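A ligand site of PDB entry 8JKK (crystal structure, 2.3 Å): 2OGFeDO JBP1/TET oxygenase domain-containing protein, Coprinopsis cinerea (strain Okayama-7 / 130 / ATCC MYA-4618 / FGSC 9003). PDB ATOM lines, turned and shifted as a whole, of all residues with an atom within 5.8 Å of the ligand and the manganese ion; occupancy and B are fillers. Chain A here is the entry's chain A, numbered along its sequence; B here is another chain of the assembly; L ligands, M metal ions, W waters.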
ATOM      1  N   TRP A 204     -33.107  38.269  15.826  1.00  0.00           N
ATOM      2  CA  TRP A 204     -31.943  38.230  14.957  1.00  0.00           C
ATOM      3  C   TRP A 204     -31.985  37.075  13.969  1.00  0.00           C
ATOM      4  O   TRP A 204     -31.383  37.160  12.888  1.00  0.00           O
ATOM      5  CB  TRP A 204     -30.670  38.192  15.811  1.00  0.00           C
ATOM      6  CG  TRP A 204     -30.439  36.881  16.486  1.00  0.00           C
ATOM      7  CD1 TRP A 204     -30.757  36.560  17.778  1.00  0.00           C
ATOM      8  CD2 TRP A 204     -29.827  35.715  15.918  1.00  0.00           C
ATOM      9  NE1 TRP A 204     -30.383  35.263  18.050  1.00  0.00           N
ATOM     10  CE2 TRP A 204     -29.797  34.729  16.937  1.00  0.00           C
ATOM     11  CE3 TRP A 204     -29.290  35.408  14.663  1.00  0.00           C
ATOM     12  CZ2 TRP A 204     -29.268  33.448  16.733  1.00  0.00           C
ATOM     13  CZ3 TRP A 204     -28.761  34.127  14.459  1.00  0.00           C
ATOM     14  CH2 TRP A 204     -28.753  33.169  15.491  1.00  0.00           C
ATOM     15  N   ARG A 205     -32.681  35.989  14.302  1.00  0.00           N
ATOM     16  CA  ARG A 205     -32.670  34.828  13.419  1.00  0.00           C
ATOM     17  C   ARG A 205     -33.295  35.108  12.058  1.00  0.00           C
ATOM     18  O   ARG A 205     -32.992  34.406  11.093  1.00  0.00           O
ATOM     19  CB  ARG A 205     -33.380  33.644  14.074  1.00  0.00           C
ATOM     20  CG  ARG A 205     -32.608  33.063  15.232  1.00  0.00           C
ATOM     21  CD  ARG A 205     -33.385  31.946  15.885  1.00  0.00           C
ATOM     22  NE  ARG A 205     -32.813  31.582  17.177  1.00  0.00           N
ATOM     23  CZ  ARG A 205     -31.721  30.833  17.324  1.00  0.00           C
ATOM     24  NH1 ARG A 205     -31.079  30.374  16.249  1.00  0.00           N
ATOM     25  NH2 ARG A 205     -31.280  30.541  18.531  1.00  0.00           N
ATOM     26  N   ILE A 318     -32.202  26.996   7.689  1.00  0.00           N
ATOM     27  CA  ILE A 318     -31.816  28.391   7.557  1.00  0.00           C
ATOM     28  C   ILE A 318     -31.220  28.543   6.157  1.00  0.00           C
ATOM     29  O   ILE A 318     -30.140  27.999   5.878  1.00  0.00           O
ATOM     30  CB  ILE A 318     -30.801  28.806   8.641  1.00  0.00           C
ATOM     31  CG1 ILE A 318     -31.372  28.616  10.048  1.00  0.00           C
ATOM     32  CG2 ILE A 318     -30.347  30.249   8.471  1.00  0.00           C
ATOM     33  CD1 ILE A 318     -31.039  27.293  10.661  1.00  0.00           C
ATOM     34  N   ARG A 321     -28.551  32.640   4.911  1.00  0.00           N
ATOM     35  CA  ARG A 321     -28.448  33.594   6.002  1.00  0.00           C
ATOM     36  C   ARG A 321     -27.106  33.462   6.702  1.00  0.00           C
ATOM     37  O   ARG A 321     -26.712  32.365   7.105  1.00  0.00           O
ATOM     38  CB  ARG A 321     -29.598  33.408   7.014  1.00  0.00           C
ATOM     39  CG  ARG A 321     -29.771  34.601   7.979  1.00  0.00           C
ATOM     40  CD  ARG A 321     -30.356  34.161   9.341  1.00  0.00           C
ATOM     41  NE  ARG A 321     -29.420  33.334  10.104  1.00  0.00           N
ATOM     42  CZ  ARG A 321     -29.778  32.450  11.023  1.00  0.00           C
ATOM     43  NH1 ARG A 321     -31.065  32.279  11.333  1.00  0.00           N
ATOM     44  NH2 ARG A 321     -28.856  31.729  11.624  1.00  0.00           N
ATOM     45  N   ALA A 322     -26.431  34.601   6.872  1.00  0.00           N
ATOM     46  CA  ALA A 322     -25.279  34.629   7.747  1.00  0.00           C
ATOM     47  C   ALA A 322     -25.736  34.504   9.204  1.00  0.00           C
ATOM     48  O   ALA A 322     -26.895  34.764   9.541  1.00  0.00           O
ATOM     49  CB  ALA A 322     -24.479  35.916   7.542  1.00  0.00           C
ATOM     50  N   THR A 323     -24.816  34.089  10.067  1.00  0.00           N
ATOM     51  CA  THR A 323     -25.134  33.790  11.456  1.00  0.00           C
ATOM     52  C   THR A 323     -24.161  34.506  12.388  1.00  0.00           C
ATOM     53  O   THR A 323     -22.988  34.091  12.491  1.00  0.00           O
ATOM     54  CB  THR A 323     -25.083  32.275  11.676  1.00  0.00           C
ATOM     55  OG1 THR A 323     -26.035  31.646  10.815  1.00  0.00           O
ATOM     56  CG2 THR A 323     -25.406  31.900  13.139  1.00  0.00           C
ATOM     57  N   HIS A 326     -23.217  33.681  18.579  1.00  0.00           N
ATOM     58  CA  HIS A 326     -24.323  33.554  19.527  1.00  0.00           C
ATOM     59  C   HIS A 326     -24.202  32.222  20.260  1.00  0.00           C
ATOM     60  O   HIS A 326     -23.452  31.336  19.874  1.00  0.00           O
ATOM     61  CB  HIS A 326     -25.678  33.606  18.814  1.00  0.00           C
ATOM     62  CG  HIS A 326     -25.967  32.352  18.048  1.00  0.00           C
ATOM     63  ND1 HIS A 326     -25.341  32.060  16.857  1.00  0.00           N
ATOM     64  CD2 HIS A 326     -26.727  31.271  18.348  1.00  0.00           C
ATOM     65  CE1 HIS A 326     -25.737  30.877  16.435  1.00  0.00           C
ATOM     66  NE2 HIS A 326     -26.574  30.369  17.329  1.00  0.00           N
ATOM     67  N   ARG A 327     -24.973  32.104  21.342  1.00  0.00           N
ATOM     68  CA  ARG A 327     -25.359  30.826  21.914  1.00  0.00           C
ATOM     69  C   ARG A 327     -26.860  30.658  21.730  1.00  0.00           C
ATOM     70  O   ARG A 327     -27.601  31.633  21.700  1.00  0.00           O
ATOM     71  CB  ARG A 327     -25.042  30.737  23.407  1.00  0.00           C
ATOM     72  CG  ARG A 327     -23.592  30.913  23.794  1.00  0.00           C
ATOM     73  CD  ARG A 327     -23.427  30.770  25.320  1.00  0.00           C
ATOM     74  NE  ARG A 327     -22.093  31.138  25.806  1.00  0.00           N
ATOM     75  CZ  ARG A 327     -21.727  32.385  26.103  1.00  0.00           C
ATOM     76  NH1 ARG A 327     -22.597  33.369  25.956  1.00  0.00           N
ATOM     77  NH2 ARG A 327     -20.505  32.654  26.562  1.00  0.00           N
ATOM     78  N   ASP A 328     -27.303  29.410  21.586  1.00  0.00           N
ATOM     79  CA  ASP A 328     -28.706  29.055  21.506  1.00  0.00           C
ATOM     80  C   ASP A 328     -29.195  28.729  22.904  1.00  0.00           C
ATOM     81  O   ASP A 328     -28.685  27.796  23.535  1.00  0.00           O
ATOM     82  CB  ASP A 328     -28.910  27.846  20.572  1.00  0.00           C
ATOM     83  CG  ASP A 328     -28.356  28.081  19.179  1.00  0.00           C
ATOM     84  OD1 ASP A 328     -28.935  28.922  18.442  1.00  0.00           O
ATOM     85  OD2 ASP A 328     -27.362  27.430  18.801  1.00  0.00           O
ATOM     86  N   LEU A 339     -25.210  20.708  13.410  1.00  0.00           N
ATOM     87  CA  LEU A 339     -25.324  21.586  12.255  1.00  0.00           C
ATOM     88  C   LEU A 339     -24.809  20.844  11.040  1.00  0.00           C
ATOM     89  O   LEU A 339     -23.775  20.171  11.108  1.00  0.00           O
ATOM     90  CB  LEU A 339     -24.482  22.847  12.474  1.00  0.00           C
ATOM     91  CG  LEU A 339     -24.784  23.583  13.787  1.00  0.00           C
ATOM     92  CD1 LEU A 339     -23.760  24.667  14.051  1.00  0.00           C
ATOM     93  CD2 LEU A 339     -26.198  24.189  13.686  1.00  0.00           C
ATOM     94  N   VAL A 340     -25.567  20.948   9.936  1.00  0.00           N
ATOM     95  CA  VAL A 340     -25.135  20.467   8.622  1.00  0.00           C
ATOM     96  C   VAL A 340     -25.208  21.653   7.678  1.00  0.00           C
ATOM     97  O   VAL A 340     -26.222  22.357   7.658  1.00  0.00           O
ATOM     98  CB  VAL A 340     -26.014  19.325   8.115  1.00  0.00           C
ATOM     99  CG1 VAL A 340     -25.419  18.716   6.832  1.00  0.00           C
ATOM    100  CG2 VAL A 340     -26.150  18.263   9.178  1.00  0.00           C
ATOM    101  N   THR A 341     -24.150  21.899   6.922  1.00  0.00           N
ATOM    102  CA  THR A 341     -24.151  23.033   5.997  1.00  0.00           C
ATOM    103  C   THR A 341     -23.991  22.547   4.562  1.00  0.00           C
ATOM    104  O   THR A 341     -23.273  21.567   4.306  1.00  0.00           O
ATOM    105  CB  THR A 341     -23.043  24.054   6.363  1.00  0.00           C
ATOM    106  OG1 THR A 341     -23.143  25.195   5.492  1.00  0.00           O
ATOM    107  CG2 THR A 341     -21.616  23.426   6.259  1.00  0.00           C
ATOM    108  N   LEU A 350     -16.735  28.614  10.293  1.00  0.00           N
ATOM    109  CA  LEU A 350     -17.470  28.650  11.541  1.00  0.00           C
ATOM    110  C   LEU A 350     -16.531  29.095  12.646  1.00  0.00           C
ATOM    111  O   LEU A 350     -15.445  28.507  12.818  1.00  0.00           O
ATOM    112  CB  LEU A 350     -18.108  27.291  11.851  1.00  0.00           C
ATOM    113  CG  LEU A 350     -19.113  27.254  13.025  1.00  0.00           C
ATOM    114  CD1 LEU A 350     -20.207  26.244  12.754  1.00  0.00           C
ATOM    115  CD2 LEU A 350     -18.380  26.803  14.233  1.00  0.00           C
ATOM    116  N   TYR A 361     -15.775  25.323   6.925  1.00  0.00           N
ATOM    117  CA  TYR A 361     -17.183  24.997   7.072  1.00  0.00           C
ATOM    118  C   TYR A 361     -17.844  25.030   5.696  1.00  0.00           C
ATOM    119  O   TYR A 361     -18.755  25.814   5.426  1.00  0.00           O
ATOM    120  CB  TYR A 361     -17.820  25.971   8.048  1.00  0.00           C
ATOM    121  CG  TYR A 361     -19.219  25.657   8.547  1.00  0.00           C
ATOM    122  CD1 TYR A 361     -19.483  24.528   9.310  1.00  0.00           C
ATOM    123  CD2 TYR A 361     -20.267  26.524   8.295  1.00  0.00           C
ATOM    124  CE1 TYR A 361     -20.773  24.268   9.778  1.00  0.00           C
ATOM    125  CE2 TYR A 361     -21.543  26.281   8.780  1.00  0.00           C
ATOM    126  CZ  TYR A 361     -21.786  25.157   9.522  1.00  0.00           C
ATOM    127  OH  TYR A 361     -23.059  24.935   9.981  1.00  0.00           O
ATOM    128  N   GLY A 371     -24.502  23.884  21.895  1.00  0.00           N
ATOM    129  CA  GLY A 371     -24.778  25.219  21.390  1.00  0.00           C
ATOM    130  C   GLY A 371     -25.267  26.220  22.437  1.00  0.00           C
ATOM    131  O   GLY A 371     -25.355  27.409  22.117  1.00  0.00           O
ATOM    132  N   HIS A 376     -20.839  30.416  18.769  1.00  0.00           N
ATOM    133  CA  HIS A 376     -20.512  30.022  17.393  1.00  0.00           C
ATOM    134  C   HIS A 376     -21.139  31.009  16.408  1.00  0.00           C
ATOM    135  O   HIS A 376     -22.190  31.588  16.685  1.00  0.00           O
ATOM    136  CB  HIS A 376     -20.982  28.597  17.064  1.00  0.00           C
ATOM    137  CG  HIS A 376     -22.430  28.340  17.388  1.00  0.00           C
ATOM    138  ND1 HIS A 376     -22.890  28.203  18.678  1.00  0.00           N
ATOM    139  CD2 HIS A 376     -23.509  28.197  16.585  1.00  0.00           C
ATOM    140  CE1 HIS A 376     -24.191  27.974  18.665  1.00  0.00           C
ATOM    141  NE2 HIS A 376     -24.595  27.967  17.410  1.00  0.00           N
ATOM    142  N   VAL A 378     -21.232  32.025  11.815  1.00  0.00           N
ATOM    143  CA  VAL A 378     -20.883  31.715  10.438  1.00  0.00           C
ATOM    144  C   VAL A 378     -21.011  32.986   9.595  1.00  0.00           C
ATOM    145  O   VAL A 378     -22.128  33.434   9.323  1.00  0.00           O
ATOM    146  CB  VAL A 378     -21.755  30.587   9.861  1.00  0.00           C
ATOM    147  CG1 VAL A 378     -21.287  30.217   8.470  1.00  0.00           C
ATOM    148  CG2 VAL A 378     -21.752  29.389  10.769  1.00  0.00           C
ATOM    149  N   ARG A 385     -25.970  29.106   0.305  1.00  0.00           N
ATOM    150  CA  ARG A 385     -25.732  28.211   1.431  1.00  0.00           C
ATOM    151  C   ARG A 385     -27.052  27.958   2.145  1.00  0.00           C
ATOM    152  O   ARG A 385     -27.951  28.809   2.143  1.00  0.00           O
ATOM    153  CB  ARG A 385     -24.712  28.824   2.395  1.00  0.00           C
ATOM    154  CG  ARG A 385     -24.478  28.048   3.662  1.00  0.00           C
ATOM    155  CD  ARG A 385     -23.345  28.622   4.473  1.00  0.00           C
ATOM    156  NE  ARG A 385     -23.832  29.565   5.460  1.00  0.00           N
ATOM    157  CZ  ARG A 385     -24.325  29.205   6.645  1.00  0.00           C
ATOM    158  NH1 ARG A 385     -24.387  27.904   6.974  1.00  0.00           N
ATOM    159  NH2 ARG A 385     -24.767  30.120   7.490  1.00  0.00           N
ATOM    160  N   TYR A 386     -27.153  26.774   2.744  1.00  0.00           N
ATOM    161  CA  TYR A 386     -28.225  26.498   3.689  1.00  0.00           C
ATOM    162  C   TYR A 386     -27.627  25.721   4.858  1.00  0.00           C
ATOM    163  O   TYR A 386     -26.566  25.103   4.747  1.00  0.00           O
ATOM    164  CB  TYR A 386     -29.378  25.700   3.073  1.00  0.00           C
ATOM    165  CG  TYR A 386     -28.945  24.357   2.527  1.00  0.00           C
ATOM    166  CD1 TYR A 386     -28.726  23.271   3.381  1.00  0.00           C
ATOM    167  CD2 TYR A 386     -28.739  24.176   1.159  1.00  0.00           C
ATOM    168  CE1 TYR A 386     -28.320  22.053   2.890  1.00  0.00           C
ATOM    169  CE2 TYR A 386     -28.332  22.955   0.647  1.00  0.00           C
ATOM    170  CZ  TYR A 386     -28.127  21.906   1.521  1.00  0.00           C
ATOM    171  OH  TYR A 386     -27.719  20.710   1.042  1.00  0.00           O
ATOM    172  N   CYS A 387     -28.347  25.754   5.976  1.00  0.00           N
ATOM    173  CA  CYS A 387     -27.947  25.048   7.191  1.00  0.00           C
ATOM    174  C   CYS A 387     -29.146  24.302   7.752  1.00  0.00           C
ATOM    175  O   CYS A 387     -30.251  24.870   7.835  1.00  0.00           O
ATOM    176  CB  CYS A 387     -27.395  26.032   8.236  1.00  0.00           C
ATOM    177  SG  CYS A 387     -27.320  25.342   9.908  1.00  0.00           S
ATOM    178  N   ALA A 389     -30.163  22.755  11.239  1.00  0.00           N
ATOM    179  CA  ALA A 389     -29.794  22.791  12.651  1.00  0.00           C
ATOM    180  C   ALA A 389     -30.755  21.905  13.432  1.00  0.00           C
ATOM    181  O   ALA A 389     -31.971  22.139  13.438  1.00  0.00           O
ATOM    182  CB  ALA A 389     -29.826  24.235  13.164  1.00  0.00           C
ATOM    183  N1  5CM B   6     -34.782  28.096  17.163  1.00  0.00           N
ATOM    184  C2  5CM B   6     -34.473  27.582  18.397  1.00  0.00           C
ATOM    185  N3  5CM B   6     -33.381  26.914  18.650  1.00  0.00           N
ATOM    186  C4  5CM B   6     -32.504  26.671  17.766  1.00  0.00           C
ATOM    187  C5  5CM B   6     -32.739  27.167  16.441  1.00  0.00           C
ATOM    188  C5A 5CM B   6     -31.702  26.907  15.377  1.00  0.00           C
ATOM    189  C6  5CM B   6     -33.901  27.877  16.190  1.00  0.00           C
ATOM    190  O2  5CM B   6     -35.194  27.713  19.337  1.00  0.00           O
ATOM    191  N4  5CM B   6     -31.435  26.002  18.113  1.00  0.00           N
ATOM    192  C1' 5CM B   6     -36.005  28.833  16.890  1.00  0.00           C
ATOM    193  C2' 5CM B   6     -37.335  28.269  17.441  1.00  0.00           C
ATOM    194  C3' 5CM B   6     -38.112  29.416  18.026  1.00  0.00           C
ATOM    195  C4' 5CM B   6     -37.047  30.492  18.022  1.00  0.00           C
ATOM    196  O4' 5CM B   6     -35.817  30.017  17.527  1.00  0.00           O
ATOM    197  O3' 5CM B   6     -38.792  29.602  16.875  1.00  0.00           O
ATOM    198  C5' 5CM B   6     -36.889  31.164  19.368  1.00  0.00           C
ATOM    199  O5' 5CM B   6     -35.889  30.734  20.227  1.00  0.00           O
ATOM    200  P   5CM B   6     -35.095  31.824  21.079  1.00  0.00           P
ATOM    201  OP1 5CM B   6     -34.486  30.998  22.111  1.00  0.00           O
ATOM    202  OP2 5CM B   6     -34.315  32.715  20.233  1.00  0.00           O
HETATM  203  C1  LIG L   1     -28.201  28.854  14.175  1.00  0.00           C
HETATM  204  C2  LIG L   1     -26.805  28.387  13.769  1.00  0.00           C
HETATM  205  C3  LIG L   1     -25.266  27.803  11.885  1.00  0.00           C
HETATM  206  C4  LIG L   1     -25.224  28.102  10.384  1.00  0.00           C
HETATM  207  O1  LIG L   1     -28.563  28.746  15.373  1.00  0.00           O
HETATM  208  O2  LIG L   1     -28.965  29.364  13.314  1.00  0.00           O
HETATM  209  O3  LIG L   1     -25.973  28.154  14.671  1.00  0.00           O
HETATM  210  O4  LIG L   1     -24.546  27.321   9.673  1.00  0.00           O
HETATM  211  N1  LIG L   1     -26.563  28.250  12.443  1.00  0.00           N
HETATM  212  O5  LIG L   1     -25.873  29.085   9.965  1.00  0.00           O
HETATM  213 MN    MN M   1     -26.948  28.296  16.709  1.00  0.00          MN
HETATM  214  O   HOH W   1     -31.451  30.444  13.344  1.00  0.00           O
HETATM  215  O   HOH W   2     -27.153  26.177  16.414  1.00  0.00           O
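An oxygen (O5) of the ligand is in hydrogen-bond range of the side-chain hydroxyl of Thr 323 (2.7 Å).
An oxygen (O4) of the ligand lies within salt-bridge range of the guanidinium group of Arg 385 (2.8 Å).
The side-chain hydroxyl (OH) of Tyr 361 sits at hydrogen-bond distance from an oxygen (O4) of the ligand (2.8 Å).
The guanidinium group (NH2) of Arg 321 is in salt-bridge range of an oxygen (O2) of the ligand (2.9 Å).
NH1 of Arg 205 is in salt-bridge range of O2 of the ligand (3.8 Å).
O4 of the ligand sits at hydrogen-bond distance from SG of Cys 387 (3.4 Å).
Three residues have an atom within 4 Å of the manganese ion: His 326, Asp 328 and His 376.
Along chain A the residues within 4 Å of the manganese ion span positions 326 to 376.
The nearest printed residue that does not touch the manganese ion is Arg 205 (4.6 Å).
Residues that only touch the ligand: Ile 318 (3.95 Å), Val 378 (3.6 Å) and 5CM 6 of chain B (3.6 Å).
Hydrophobic or aromatic side chains that line the ligand: Ile 318, His 326, Tyr 361, His 376 and Val 378.
The nearest printed residue that does not touch the ligand is Leu 339 (4.1 Å).
The guanidinium group of Arg 205 is in salt-bridge range of the side-chain carboxylate of Asp 328, 2.9 Å away.
The backbone carbonyl oxygen (O) of Gly 371 sits at hydrogen-bond distance from the backbone NH (N) of Asp 328 (2.8 Å).
OG1 of Thr 323 is in hydrogen-bond range of NH2 of Arg 321 (2.9 Å).
The backbone carbonyl oxygen (O) of Thr 323 is in hydrogen-bond range of the backbone NH (N) of Val 378 (2.8 Å).
The side-chain hydroxyl (OG1) of Thr 341 is in hydrogen-bond range of the guanidinium group (NH1) of Arg 385, at 3.3 Å.
The guanidinium group (NH1) of Arg 321 lies within hydrogen-bond range of the backbone carbonyl oxygen (O) of Arg 205 (2.9 Å).
OP2 of 5CM 6 of chain B is in salt-bridge range of NE of Arg 205 (3.6 Å).
The backbone carbonyl oxygen of Ile 318 sits at hydrogen-bond distance from the backbone NH of Cys 387, at 2.9 Å.
The manganese ion is bound by O1 of the ligand (2.1 Å).
Water W2 binds the manganese ion (2.1 Å).
A ring nitrogen (NE2) of His 326 binds the manganese ion (2.2 Å).
O3 of the ligand is bound to the manganese ion (2.3 Å).
OD2 of Asp 328 binds the manganese ion (2.3 Å).
NE2 of His 376 binds the manganese ion (2.5 Å).
Slightly farther from the manganese ion lies OD1 of Asp 328 (2.7 Å).
Water W1 lies within hydrogen-bond range of an oxygen (O2) of the ligand (2.7 Å), the guanidinium group (NH1) of Arg 321 (2.7 Å) and the guanidinium group (NH1) of Arg 205 (2.9 Å).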
